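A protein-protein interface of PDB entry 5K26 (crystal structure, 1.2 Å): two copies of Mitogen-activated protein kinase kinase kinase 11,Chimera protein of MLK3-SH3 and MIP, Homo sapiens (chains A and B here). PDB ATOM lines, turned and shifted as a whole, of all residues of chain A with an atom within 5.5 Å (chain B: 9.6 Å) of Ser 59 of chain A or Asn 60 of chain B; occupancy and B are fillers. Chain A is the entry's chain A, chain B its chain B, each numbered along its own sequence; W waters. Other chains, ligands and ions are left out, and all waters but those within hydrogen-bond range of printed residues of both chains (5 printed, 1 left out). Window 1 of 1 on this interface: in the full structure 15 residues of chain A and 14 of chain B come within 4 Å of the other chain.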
ATOM      1  N   GLU A  43      10.134 -23.286 -28.797  1.00  0.00           N
ATOM      2  CA  GLU A  43       9.680 -24.483 -28.102  1.00  0.00           C
ATOM      3  C   GLU A  43       8.514 -24.102 -27.190  1.00  0.00           C
ATOM      4  O   GLU A  43       8.575 -23.065 -26.533  1.00  0.00           O
ATOM      5  CB  GLU A  43      10.808 -25.140 -27.321  1.00  0.00           C
ATOM      6  CG  GLU A  43      10.467 -26.465 -26.722  1.00  0.00           C
ATOM      7  CD  GLU A  43      10.301 -27.580 -27.714  1.00  0.00           C
ATOM      8  OE1 GLU A  43      10.988 -27.613 -28.696  1.00  0.00           O
ATOM      9  OE2 GLU A  43       9.366 -28.497 -27.485  1.00  0.00           O
ATOM     10  N   GLY A  44       7.546 -24.973 -27.125  1.00  0.00           N
ATOM     11  CA  GLY A  44       6.379 -24.683 -26.343  1.00  0.00           C
ATOM     12  C   GLY A  44       5.143 -24.268 -27.258  1.00  0.00           C
ATOM     13  O   GLY A  44       4.080 -24.308 -26.779  1.00  0.00           O
ATOM     14  N   TRP A  45       5.458 -23.926 -28.487  1.00  0.00           N
ATOM     15  CA  TRP A  45       4.439 -23.646 -29.513  1.00  0.00           C
ATOM     16  C   TRP A  45       4.332 -24.802 -30.366  1.00  0.00           C
ATOM     17  O   TRP A  45       5.375 -25.389 -30.827  1.00  0.00           O
ATOM     18  CB  TRP A  45       4.831 -22.313 -30.214  1.00  0.00           C
ATOM     19  CG  TRP A  45       4.669 -21.142 -29.393  1.00  0.00           C
ATOM     20  CD1 TRP A  45       5.486 -20.761 -28.346  1.00  0.00           C
ATOM     21  CD2 TRP A  45       3.587 -20.195 -29.434  1.00  0.00           C
ATOM     22  NE1 TRP A  45       4.976 -19.643 -27.779  1.00  0.00           N
ATOM     23  CE2 TRP A  45       3.852 -19.285 -28.455  1.00  0.00           C
ATOM     24  CE3 TRP A  45       2.491 -20.004 -30.295  1.00  0.00           C
ATOM     25  CZ2 TRP A  45       2.994 -18.154 -28.223  1.00  0.00           C
ATOM     26  CZ3 TRP A  45       1.715 -18.923 -30.119  1.00  0.00           C
ATOM     27  CH2 TRP A  45       1.966 -18.013 -29.110  1.00  0.00           C
ATOM     28  N   TRP A  46       3.109 -25.294 -30.629  1.00  0.00           N
ATOM     29  CA  TRP A  46       2.848 -26.435 -31.380  1.00  0.00           C
ATOM     30  C   TRP A  46       2.137 -26.043 -32.777  1.00  0.00           C
ATOM     31  O   TRP A  46       1.509 -24.943 -32.773  1.00  0.00           O
ATOM     32  CB  TRP A  46       1.933 -27.391 -30.698  1.00  0.00           C
ATOM     33  CG  TRP A  46       2.609 -28.063 -29.443  1.00  0.00           C
ATOM     34  CD1 TRP A  46       3.889 -27.854 -29.067  1.00  0.00           C
ATOM     35  CD2 TRP A  46       1.966 -28.875 -28.496  1.00  0.00           C
ATOM     36  NE1 TRP A  46       4.097 -28.598 -27.870  1.00  0.00           N
ATOM     37  CE2 TRP A  46       2.995 -29.224 -27.499  1.00  0.00           C
ATOM     38  CE3 TRP A  46       0.706 -29.351 -28.343  1.00  0.00           C
ATOM     39  CZ2 TRP A  46       2.679 -29.999 -26.397  1.00  0.00           C
ATOM     40  CZ3 TRP A  46       0.389 -30.173 -27.231  1.00  0.00           C
ATOM     41  CH2 TRP A  46       1.415 -30.488 -26.308  1.00  0.00           C
ATOM     42  N   PHE A  57       0.315 -22.398 -31.970  1.00  0.00           N
ATOM     43  CA  PHE A  57      -0.436 -22.028 -30.878  1.00  0.00           C
ATOM     44  C   PHE A  57       0.273 -22.407 -29.516  1.00  0.00           C
ATOM     45  O   PHE A  57       1.152 -23.382 -29.619  1.00  0.00           O
ATOM     46  CB  PHE A  57      -1.828 -22.662 -30.872  1.00  0.00           C
ATOM     47  CG  PHE A  57      -1.865 -24.125 -30.840  1.00  0.00           C
ATOM     48  CD1 PHE A  57      -1.758 -24.905 -31.927  1.00  0.00           C
ATOM     49  CD2 PHE A  57      -1.908 -24.822 -29.613  1.00  0.00           C
ATOM     50  CE1 PHE A  57      -1.666 -26.346 -31.870  1.00  0.00           C
ATOM     51  CE2 PHE A  57      -1.787 -26.230 -29.547  1.00  0.00           C
ATOM     52  CZ  PHE A  57      -1.685 -26.956 -30.640  1.00  0.00           C
ATOM     53  N   PRO A  58      -0.040 -21.826 -28.479  1.00  0.00           N
ATOM     54  CA  PRO A  58       0.721 -22.199 -27.202  1.00  0.00           C
ATOM     55  C   PRO A  58       0.098 -23.447 -26.701  1.00  0.00           C
ATOM     56  O   PRO A  58      -1.077 -23.648 -26.417  1.00  0.00           O
ATOM     57  CB  PRO A  58       0.358 -20.970 -26.300  1.00  0.00           C
ATOM     58  CG  PRO A  58      -0.883 -20.346 -26.894  1.00  0.00           C
ATOM     59  CD  PRO A  58      -0.891 -20.647 -28.333  1.00  0.00           C
ATOM     60  N   SER A  59       1.047 -24.402 -26.330  1.00  0.00           N
ATOM     61  CA  SER A  59       0.652 -25.750 -25.917  1.00  0.00           C
ATOM     62  C   SER A  59      -0.107 -25.757 -24.612  1.00  0.00           C
ATOM     63  O   SER A  59      -0.834 -26.698 -24.472  1.00  0.00           O
ATOM     64  CB  SER A  59       1.886 -26.652 -25.846  1.00  0.00           C
ATOM     65  OG  SER A  59       2.809 -26.134 -24.894  1.00  0.00           O
ATOM     66  N   ASN A  60       0.081 -24.820 -23.778  1.00  0.00           N
ATOM     67  CA  ASN A  60      -0.610 -24.794 -22.539  1.00  0.00           C
ATOM     68  C   ASN A  60      -2.129 -24.435 -22.550  1.00  0.00           C
ATOM     69  O   ASN A  60      -2.820 -24.400 -21.642  1.00  0.00           O
ATOM     70  CB  ASN A  60       0.080 -23.919 -21.478  1.00  0.00           C
ATOM     71  CG  ASN A  60       0.392 -22.514 -21.989  1.00  0.00           C
ATOM     72  OD1 ASN A  60       0.621 -22.274 -23.123  1.00  0.00           O
ATOM     73  ND2 ASN A  60       0.624 -21.606 -21.044  1.00  0.00           N
ATOM     74  N   TYR A  61      -2.571 -24.167 -23.847  1.00  0.00           N
ATOM     75  CA  TYR A  61      -3.999 -23.844 -24.119  1.00  0.00           C
ATOM     76  C   TYR A  61      -4.739 -24.994 -24.558  1.00  0.00           C
ATOM     77  O   TYR A  61      -5.967 -24.855 -24.808  1.00  0.00           O
ATOM     78  CB  TYR A  61      -4.070 -22.639 -25.108  1.00  0.00           C
ATOM     79  CG  TYR A  61      -3.802 -21.306 -24.503  1.00  0.00           C
ATOM     80  CD1 TYR A  61      -2.626 -21.004 -23.875  1.00  0.00           C
ATOM     81  CD2 TYR A  61      -4.855 -20.318 -24.514  1.00  0.00           C
ATOM     82  CE1 TYR A  61      -2.438 -19.732 -23.372  1.00  0.00           C
ATOM     83  CE2 TYR A  61      -4.609 -19.115 -24.002  1.00  0.00           C
ATOM     84  CZ  TYR A  61      -3.446 -18.816 -23.433  1.00  0.00           C
ATOM     85  OH  TYR A  61      -3.228 -17.543 -22.852  1.00  0.00           O
ATOM     86  N   VAL A  62      -4.185 -26.206 -24.680  1.00  0.00           N
ATOM     87  CA  VAL A  62      -4.890 -27.348 -25.140  1.00  0.00           C
ATOM     88  C   VAL A  62      -4.745 -28.520 -24.131  1.00  0.00           C
ATOM     89  O   VAL A  62      -3.787 -28.562 -23.348  1.00  0.00           O
ATOM     90  CB  VAL A  62      -4.488 -27.822 -26.538  1.00  0.00           C
ATOM     91  CG1 VAL A  62      -4.850 -26.733 -27.621  1.00  0.00           C
ATOM     92  CG2 VAL A  62      -3.034 -28.174 -26.605  1.00  0.00           C
ATOM     93  N   TRP B   8       4.872 -24.116  -9.713  1.00  0.00           N
ATOM     94  CA  TRP B   8       4.238 -24.456 -10.923  1.00  0.00           C
ATOM     95  C   TRP B   8       4.299 -25.978 -11.066  1.00  0.00           C
ATOM     96  O   TRP B   8       5.146 -26.647 -10.412  1.00  0.00           O
ATOM     97  CB  TRP B   8       4.911 -23.755 -12.072  1.00  0.00           C
ATOM     98  CG  TRP B   8       4.772 -22.225 -12.065  1.00  0.00           C
ATOM     99  CD1 TRP B   8       5.296 -21.322 -11.062  1.00  0.00           C
ATOM    100  CD2 TRP B   8       4.140 -21.439 -12.969  1.00  0.00           C
ATOM    101  NE1 TRP B   8       5.001 -20.084 -11.386  1.00  0.00           N
ATOM    102  CE2 TRP B   8       4.257 -20.060 -12.551  1.00  0.00           C
ATOM    103  CE3 TRP B   8       3.465 -21.709 -14.137  1.00  0.00           C
ATOM    104  CZ2 TRP B   8       3.764 -19.021 -13.203  1.00  0.00           C
ATOM    105  CZ3 TRP B   8       2.920 -20.637 -14.872  1.00  0.00           C
ATOM    106  CH2 TRP B   8       3.051 -19.277 -14.441  1.00  0.00           C
ATOM    107  N   THR B   9       3.492 -26.551 -11.941  1.00  0.00           N
ATOM    108  CA  THR B   9       3.464 -27.932 -12.272  1.00  0.00           C
ATOM    109  C   THR B   9       3.772 -28.151 -13.669  1.00  0.00           C
ATOM    110  O   THR B   9       3.202 -27.465 -14.558  1.00  0.00           O
ATOM    111  CB  THR B   9       2.108 -28.490 -11.869  1.00  0.00           C
ATOM    112  OG1 THR B   9       1.860 -28.263 -10.464  1.00  0.00           O
ATOM    113  CG2 THR B   9       2.056 -29.917 -12.077  1.00  0.00           C
ATOM    114  N   ALA B  10       4.635 -29.131 -14.030  1.00  0.00           N
ATOM    115  CA  ALA B  10       4.836 -29.484 -15.433  1.00  0.00           C
ATOM    116  C   ALA B  10       3.678 -30.164 -16.014  1.00  0.00           C
ATOM    117  O   ALA B  10       3.043 -31.046 -15.474  1.00  0.00           O
ATOM    118  CB  ALA B  10       6.066 -30.395 -15.538  1.00  0.00           C
ATOM    119  N   LEU B  11       3.301 -29.647 -17.206  1.00  0.00           N
ATOM    120  CA  LEU B  11       2.153 -30.195 -17.961  1.00  0.00           C
ATOM    121  C   LEU B  11       2.462 -31.374 -18.809  1.00  0.00           C
ATOM    122  O   LEU B  11       1.594 -32.174 -19.101  1.00  0.00           O
ATOM    123  CB  LEU B  11       1.623 -29.066 -18.939  1.00  0.00           C
ATOM    124  CG  LEU B  11       1.035 -27.861 -18.164  1.00  0.00           C
ATOM    125  CD1 LEU B  11       0.678 -26.764 -19.176  1.00  0.00           C
ATOM    126  CD2 LEU B  11      -0.272 -28.369 -17.528  1.00  0.00           C
ATOM    127  N   PHE B  12       3.687 -31.468 -19.269  1.00  0.00           N
ATOM    128  CA  PHE B  12       4.132 -32.464 -20.278  1.00  0.00           C
ATOM    129  C   PHE B  12       5.504 -32.952 -19.961  1.00  0.00           C
ATOM    130  O   PHE B  12       6.276 -32.255 -19.302  1.00  0.00           O
ATOM    131  CB  PHE B  12       4.165 -31.861 -21.676  1.00  0.00           C
ATOM    132  CG  PHE B  12       2.943 -31.065 -22.101  1.00  0.00           C
ATOM    133  CD1 PHE B  12       1.692 -31.650 -22.250  1.00  0.00           C
ATOM    134  CD2 PHE B  12       3.013 -29.761 -22.275  1.00  0.00           C
ATOM    135  CE1 PHE B  12       0.574 -30.889 -22.613  1.00  0.00           C
ATOM    136  CE2 PHE B  12       1.892 -28.991 -22.675  1.00  0.00           C
ATOM    137  CZ  PHE B  12       0.716 -29.531 -22.746  1.00  0.00           C
ATOM    138  N   ASP B  13       5.786 -34.194 -20.385  1.00  0.00           N
ATOM    139  CA  ASP B  13       7.195 -34.654 -20.436  1.00  0.00           C
ATOM    140  C   ASP B  13       7.970 -33.787 -21.449  1.00  0.00           C
ATOM    141  O   ASP B  13       7.499 -33.501 -22.549  1.00  0.00           O
ATOM    142  CB  ASP B  13       7.189 -36.107 -20.836  1.00  0.00           C
ATOM    143  CG  ASP B  13       6.564 -37.047 -19.854  1.00  0.00           C
ATOM    144  OD1 ASP B  13       6.407 -36.757 -18.632  1.00  0.00           O
ATOM    145  OD2 ASP B  13       6.381 -38.234 -20.309  1.00  0.00           O
ATOM    146  N   TYR B  14       9.191 -33.405 -21.099  1.00  0.00           N
ATOM    147  CA  TYR B  14      10.064 -32.705 -22.034  1.00  0.00           C
ATOM    148  C   TYR B  14      11.485 -33.218 -21.836  1.00  0.00           C
ATOM    149  O   TYR B  14      11.993 -33.120 -20.722  1.00  0.00           O
ATOM    150  CB  TYR B  14      10.004 -31.141 -21.748  1.00  0.00           C
ATOM    151  CG  TYR B  14      10.901 -30.337 -22.682  1.00  0.00           C
ATOM    152  CD1 TYR B  14      10.771 -30.449 -24.050  1.00  0.00           C
ATOM    153  CD2 TYR B  14      12.076 -29.772 -22.144  1.00  0.00           C
ATOM    154  CE1 TYR B  14      11.605 -29.728 -24.882  1.00  0.00           C
ATOM    155  CE2 TYR B  14      12.971 -29.077 -23.016  1.00  0.00           C
ATOM    156  CZ  TYR B  14      12.739 -29.057 -24.355  1.00  0.00           C
ATOM    157  OH  TYR B  14      13.667 -28.466 -25.217  1.00  0.00           O
ATOM    158  N   LEU B  24      11.714 -32.211 -17.843  1.00  0.00           N
ATOM    159  CA  LEU B  24      10.436 -32.216 -17.176  1.00  0.00           C
ATOM    160  C   LEU B  24       9.731 -33.495 -17.343  1.00  0.00           C
ATOM    161  O   LEU B  24       9.789 -34.103 -18.437  1.00  0.00           O
ATOM    162  CB  LEU B  24       9.484 -31.064 -17.741  1.00  0.00           C
ATOM    163  CG  LEU B  24      10.116 -29.674 -17.710  1.00  0.00           C
ATOM    164  CD1 LEU B  24       9.151 -28.684 -18.432  1.00  0.00           C
ATOM    165  CD2 LEU B  24      10.327 -29.198 -16.296  1.00  0.00           C
ATOM    166  N   VAL B  32       9.637 -21.526 -10.083  1.00  0.00           N
ATOM    167  CA  VAL B  32       9.962 -20.558 -11.140  1.00  0.00           C
ATOM    168  C   VAL B  32      10.733 -19.402 -10.531  1.00  0.00           C
ATOM    169  O   VAL B  32      10.249 -18.810  -9.560  1.00  0.00           O
ATOM    170  CB  VAL B  32       8.709 -20.111 -11.941  1.00  0.00           C
ATOM    171  CG1 VAL B  32       9.061 -18.990 -12.906  1.00  0.00           C
ATOM    172  CG2 VAL B  32       8.170 -21.278 -12.666  1.00  0.00           C
ATOM    173  N   GLU B  43      13.333 -15.498 -25.372  1.00  0.00           N
ATOM    174  CA  GLU B  43      12.002 -15.228 -24.933  1.00  0.00           C
ATOM    175  C   GLU B  43      11.183 -16.596 -25.254  1.00  0.00           C
ATOM    176  O   GLU B  43      11.373 -17.355 -26.351  1.00  0.00           O
ATOM    177  CB  GLU B  43      11.408 -14.036 -25.696  1.00  0.00           C
ATOM    178  CG  GLU B  43       9.911 -13.752 -25.466  1.00  0.00           C
ATOM    179  CD  GLU B  43       9.205 -12.784 -26.527  1.00  0.00           C
ATOM    180  OE1 GLU B  43       9.868 -12.110 -27.353  1.00  0.00           O
ATOM    181  OE2 GLU B  43       7.937 -12.758 -26.572  1.00  0.00           O
ATOM    182  N   GLY B  44      10.337 -16.849 -24.318  1.00  0.00           N
ATOM    183  CA  GLY B  44       9.539 -18.015 -24.252  1.00  0.00           C
ATOM    184  C   GLY B  44      10.041 -19.052 -23.298  1.00  0.00           C
ATOM    185  O   GLY B  44       9.323 -19.942 -22.907  1.00  0.00           O
ATOM    186  N   TRP B  45      11.289 -18.860 -22.867  1.00  0.00           N
ATOM    187  CA  TRP B  45      11.917 -19.803 -21.864  1.00  0.00           C
ATOM    188  C   TRP B  45      11.994 -19.035 -20.532  1.00  0.00           C
ATOM    189  O   TRP B  45      12.315 -17.889 -20.461  1.00  0.00           O
ATOM    190  CB  TRP B  45      13.319 -20.212 -22.376  1.00  0.00           C
ATOM    191  CG  TRP B  45      13.273 -21.155 -23.543  1.00  0.00           C
ATOM    192  CD1 TRP B  45      12.920 -20.885 -24.844  1.00  0.00           C
ATOM    193  CD2 TRP B  45      13.585 -22.547 -23.512  1.00  0.00           C
ATOM    194  NE1 TRP B  45      13.004 -22.007 -25.599  1.00  0.00           N
ATOM    195  CE2 TRP B  45      13.436 -23.055 -24.828  1.00  0.00           C
ATOM    196  CE3 TRP B  45      14.051 -23.409 -22.521  1.00  0.00           C
ATOM    197  CZ2 TRP B  45      13.715 -24.351 -25.138  1.00  0.00           C
ATOM    198  CZ3 TRP B  45      14.312 -24.702 -22.815  1.00  0.00           C
ATOM    199  CH2 TRP B  45      14.122 -25.189 -24.105  1.00  0.00           C
ATOM    200  N   TRP B  46      11.753 -19.840 -19.465  1.00  0.00           N
ATOM    201  CA  TRP B  46      11.776 -19.358 -18.144  1.00  0.00           C
ATOM    202  C   TRP B  46      12.968 -20.047 -17.358  1.00  0.00           C
ATOM    203  O   TRP B  46      13.398 -21.105 -17.806  1.00  0.00           O
ATOM    204  CB  TRP B  46      10.521 -19.680 -17.414  1.00  0.00           C
ATOM    205  CG  TRP B  46       9.313 -18.801 -17.864  1.00  0.00           C
ATOM    206  CD1 TRP B  46       9.342 -17.825 -18.781  1.00  0.00           C
ATOM    207  CD2 TRP B  46       7.998 -18.872 -17.377  1.00  0.00           C
ATOM    208  NE1 TRP B  46       8.050 -17.294 -18.863  1.00  0.00           N
ATOM    209  CE2 TRP B  46       7.230 -17.892 -18.038  1.00  0.00           C
ATOM    210  CE3 TRP B  46       7.386 -19.702 -16.443  1.00  0.00           C
ATOM    211  CZ2 TRP B  46       5.901 -17.735 -17.837  1.00  0.00           C
ATOM    212  CZ3 TRP B  46       6.019 -19.505 -16.237  1.00  0.00           C
ATOM    213  CH2 TRP B  46       5.315 -18.491 -16.910  1.00  0.00           C
ATOM    214  N   PHE B  57      13.550 -23.734 -19.036  1.00  0.00           N
ATOM    215  CA  PHE B  57      12.539 -24.603 -19.629  1.00  0.00           C
ATOM    216  C   PHE B  57      11.505 -23.763 -20.396  1.00  0.00           C
ATOM    217  O   PHE B  57      11.360 -22.560 -20.161  1.00  0.00           O
ATOM    218  CB  PHE B  57      11.824 -25.447 -18.551  1.00  0.00           C
ATOM    219  CG  PHE B  57      11.208 -24.672 -17.486  1.00  0.00           C
ATOM    220  CD1 PHE B  57      11.971 -24.323 -16.431  1.00  0.00           C
ATOM    221  CD2 PHE B  57       9.894 -24.183 -17.606  1.00  0.00           C
ATOM    222  CE1 PHE B  57      11.488 -23.511 -15.473  1.00  0.00           C
ATOM    223  CE2 PHE B  57       9.417 -23.378 -16.649  1.00  0.00           C
ATOM    224  CZ  PHE B  57      10.207 -23.045 -15.609  1.00  0.00           C
ATOM    225  N   PRO B  58      10.777 -24.405 -21.303  1.00  0.00           N
ATOM    226  CA  PRO B  58       9.701 -23.621 -22.068  1.00  0.00           C
ATOM    227  C   PRO B  58       8.582 -23.302 -21.144  1.00  0.00           C
ATOM    228  O   PRO B  58       7.985 -24.112 -20.500  1.00  0.00           O
ATOM    229  CB  PRO B  58       9.322 -24.681 -23.162  1.00  0.00           C
ATOM    230  CG  PRO B  58      10.483 -25.661 -23.241  1.00  0.00           C
ATOM    231  CD  PRO B  58      10.870 -25.752 -21.830  1.00  0.00           C
ATOM    232  N   SER B  59       8.221 -21.957 -21.182  1.00  0.00           N
ATOM    233  CA  SER B  59       7.166 -21.472 -20.339  1.00  0.00           C
ATOM    234  C   SER B  59       5.847 -22.199 -20.504  1.00  0.00           C
ATOM    235  O   SER B  59       5.107 -22.352 -19.603  1.00  0.00           O
ATOM    236  CB  SER B  59       7.028 -20.014 -20.574  1.00  0.00           C
ATOM    237  OG  SER B  59       6.587 -19.680 -21.842  1.00  0.00           O
ATOM    238  N   ASN B  60       5.584 -22.608 -21.770  1.00  0.00           N
ATOM    239  CA  ASN B  60       4.288 -23.161 -22.066  1.00  0.00           C
ATOM    240  C   ASN B  60       4.057 -24.591 -21.545  1.00  0.00           C
ATOM    241  O   ASN B  60       3.036 -25.197 -21.631  1.00  0.00           O
ATOM    242  CB  ASN B  60       4.027 -23.041 -23.541  1.00  0.00           C
ATOM    243  CG  ASN B  60       3.806 -21.625 -23.986  1.00  0.00           C
ATOM    244  OD1 ASN B  60       3.704 -20.711 -23.223  1.00  0.00           O
ATOM    245  ND2 ASN B  60       3.705 -21.474 -25.291  1.00  0.00           N
ATOM    246  N   TYR B  61       5.201 -25.199 -20.954  1.00  0.00           N
ATOM    247  CA  TYR B  61       5.143 -26.555 -20.410  1.00  0.00           C
ATOM    248  C   TYR B  61       4.838 -26.580 -18.975  1.00  0.00           C
ATOM    249  O   TYR B  61       4.922 -27.704 -18.358  1.00  0.00           O
ATOM    250  CB  TYR B  61       6.365 -27.328 -20.822  1.00  0.00           C
ATOM    251  CG  TYR B  61       6.461 -27.588 -22.324  1.00  0.00           C
ATOM    252  CD1 TYR B  61       5.370 -27.386 -23.239  1.00  0.00           C
ATOM    253  CD2 TYR B  61       7.636 -28.029 -22.879  1.00  0.00           C
ATOM    254  CE1 TYR B  61       5.564 -27.679 -24.532  1.00  0.00           C
ATOM    255  CE2 TYR B  61       7.828 -28.223 -24.188  1.00  0.00           C
ATOM    256  CZ  TYR B  61       6.735 -28.047 -25.062  1.00  0.00           C
ATOM    257  OH  TYR B  61       6.854 -28.305 -26.405  1.00  0.00           O
ATOM    258  N   VAL B  62       4.509 -25.518 -18.327  1.00  0.00           N
ATOM    259  CA  VAL B  62       4.121 -25.457 -16.975  1.00  0.00           C
ATOM    260  C   VAL B  62       2.794 -24.724 -16.716  1.00  0.00           C
ATOM    261  O   VAL B  62       2.423 -23.855 -17.565  1.00  0.00           O
ATOM    262  CB  VAL B  62       5.201 -24.845 -16.026  1.00  0.00           C
ATOM    263  CG1 VAL B  62       6.458 -25.736 -16.048  1.00  0.00           C
ATOM    264  CG2 VAL B  62       5.562 -23.420 -16.397  1.00  0.00           C
ATOM    265  N   SER B  63       2.149 -24.953 -15.627  1.00  0.00           N
ATOM    266  CA  SER B  63       1.009 -24.250 -15.189  1.00  0.00           C
ATOM    267  C   SER B  63       1.103 -23.836 -13.753  1.00  0.00           C
ATOM    268  O   SER B  63       1.718 -24.570 -12.942  1.00  0.00           O
ATOM    269  CB  SER B  63      -0.285 -25.089 -15.429  1.00  0.00           C
ATOM    270  OG  SER B  63      -0.462 -26.131 -14.588  1.00  0.00           O
ATOM    271  N   ARG B  64       0.516 -22.735 -13.363  1.00  0.00           N
ATOM    272  CA  ARG B  64       0.799 -22.255 -12.032  1.00  0.00           C
ATOM    273  C   ARG B  64      -0.077 -22.922 -11.007  1.00  0.00           C
ATOM    274  O   ARG B  64      -1.307 -23.045 -11.200  1.00  0.00           O
ATOM    275  CB  ARG B  64       0.559 -20.762 -12.030  1.00  0.00           C
ATOM    276  CG  ARG B  64       0.713 -20.029 -10.674  1.00  0.00           C
ATOM    277  CD  ARG B  64       1.991 -19.838  -9.999  1.00  0.00           C
ATOM    278  NE  ARG B  64       1.966 -18.971  -8.828  1.00  0.00           N
ATOM    279  CZ  ARG B  64       2.032 -19.410  -7.560  1.00  0.00           C
ATOM    280  NH1 ARG B  64       2.042 -20.723  -7.277  1.00  0.00           N
ATOM    281  NH2 ARG B  64       2.087 -18.543  -6.585  1.00  0.00           N
ATOM    282  N   PRO B  73      -3.408 -19.846 -17.885  1.00  0.00           N
ATOM    283  CA  PRO B  73      -2.665 -18.843 -18.598  1.00  0.00           C
ATOM    284  C   PRO B  73      -3.475 -17.742 -19.199  1.00  0.00           C
ATOM    285  O   PRO B  73      -2.879 -16.758 -19.573  1.00  0.00           O
ATOM    286  CB  PRO B  73      -1.934 -19.621 -19.666  1.00  0.00           C
ATOM    287  CG  PRO B  73      -2.783 -20.839 -19.877  1.00  0.00           C
ATOM    288  CD  PRO B  73      -3.304 -21.151 -18.518  1.00  0.00           C
HETATM  289  O   HOH W   1       1.147 -18.979 -21.752  1.00  0.00           O
HETATM  290  O   HOH W   2       7.477 -26.840 -29.481  1.00  0.00           O
HETATM  291  O   HOH W   3       6.342 -18.950 -25.193  1.00  0.00           O
HETATM  292  O   HOH W   4       7.257 -21.808 -24.287  1.00  0.00           O
HETATM  293  O   HOH W   5      -0.041 -22.692 -18.198  1.00  0.00           O
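Hydrophobic or aromatic side chains of chain A within 4 Å of the printed part of chain B: Trp 45, Trp 46, Pro 58 and Tyr 61. Of the 22 printed residues of chain B, 8 touch a printed residue of chain A. Hydrophobic or aromatic side chains of chain B that line the printed part of chain A: Leu 11, Phe 12, Tyr 14, Trp 45, Pro 58, Tyr 61 and Pro 73. Among the printed residues, 17 pairs touch across the chains. Among the printed residues, no Asp or Glu carboxylate lies within 4 Å of a Lys or Arg side-chain nitrogen of the other chain.
Glu 43 of chain A touches Pro 58 of chain B, but with the chains exchanged Pro 58 of chain A does not touch Glu 43 of chain B (11.2 Å). Gly 44 of chain A touches Tyr 61 of chain B, but with the chains exchanged Tyr 61 of chain A does not touch Gly 44 of chain B (11.8 Å). Trp 46 of chain A touches Tyr 61 of chain B, but with the chains exchanged Tyr 61 of chain A does not touch Trp 46 of chain B (10.2 Å). Positions printed for both chains: 43, 44, 45, 46, 57, 58, 59, 60, 61 and 62.
OE2 of Glu 43 of chain A sits at hydrogen-bond distance from OH of Tyr 61 of chain B, 2.7 Å away. O of Gly 44 of chain A lies within hydrogen-bond range of ND2 of Asn 60 of chain B, at 3.2 Å. N of Gly 44 of chain A lies within hydrogen-bond range of OH of Tyr 61 of chain B (3.5 Å). The indole nitrogen of Trp 45 of chain A sits close to the side-chain amide nitrogen of Asn 60 of chain B (3.3 Å). NE1 of Trp 46 of chain A sits at hydrogen-bond distance from OH of Tyr 61 of chain B (3.1 Å). O of Asn 60 of chain B sits at hydrogen-bond distance from OG of Ser 59 of chain A (3.4 Å). The side-chain amide oxygen (OD1) of Asn 60 of chain A lies close to the side-chain amide oxygen (OD1) of Asn 60 of chain B. OH of Tyr 61 of chain A sits at hydrogen-bond distance from O of Pro 73 of chain B.
Water W1 lies within hydrogen-bond range of ND2 of Asn 60 of chain A (2.8 Å) and OD1 of Asn 60 of chain B (3.4 Å). Water W4 lies within hydrogen-bond range of O of Glu 43 of chain A (2.9 Å), O of Gly 44 of chain B (3.1 Å), N of Asn 60 of chain B (3.1 Å) and N of Ser 59 of chain B (3.3 Å). Water W3 bridges the indole nitrogen of Trp 45 of chain A and the side-chain hydroxyl of Ser 59 of chain B.
OG of Ser 59 of chain A lies within hydrogen-bond range of O of Gly 44 of chain A (2.9 Å). The backbone carbonyl oxygen of Phe 57 of chain A is in hydrogen-bond range of the backbone NH of Trp 46 of chain A, at 2.9 Å. The backbone NH (N) of Leu 11 of chain B is in hydrogen-bond range of the backbone carbonyl oxygen (O) of Tyr 61 of chain B, at 2.8 Å. The backbone carbonyl oxygen (O) of Leu 24 of chain B lies within hydrogen-bond range of the backbone NH (N) of Tyr 14 of chain B.
Among the printed residues, merely in contact across the chains: Ser 59 of chain A with Tyr 61 of chain B (3.2 Å), Asn 60 of chain A with Pro 73 of chain B (3.5 Å), Pro 58 of chain A with Asn 60 of chain B (3.5 Å), Glu 43 of chain A with Pro 58 of chain B (3.6 Å), Glu 43 of chain A with Tyr 14 of chain B (3.6 Å), Ser 59 of chain A with Phe 12 of chain B (3.7 Å), Asn 60 of chain A with Leu 11 of chain B (3.7 Å), Glu 43 of chain A with Trp 45 of chain B (3.7 Å) and Trp 46 of chain A with Phe 12 of chain B (3.8 Å).
Of the printed residues of chain A, Leu 11 of chain B touches Asn 60. Printed residues of chain A within 4 Å of Phe 12 of chain B: Trp 46 and Ser 59. Val 32 of chain B touches none of the printed residues of chain A. Gly 44 of chain B touches none of the printed residues of chain A. Printed residues of chain A within 4 Å of Asn 60 of chain B: Gly 44, Trp 45, Pro 58, Ser 59 and Asn 60. Printed residues of chain A within 4 Å of Pro 73 of chain B: Asn 60 (3.5 Å) and Tyr 61 (3.4 Å). The nearest printed residue of chain B that does not touch Ser 59 of chain A is Leu 11 of chain B (5.5 Å). The nearest printed residue of chain A that does not touch Asn 60 of chain B is Glu 43 of chain A (5.3 Å). The nearest printed residue of chain A that does not touch Pro 58 of chain B is Gly 44 of chain A (4.3 Å).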
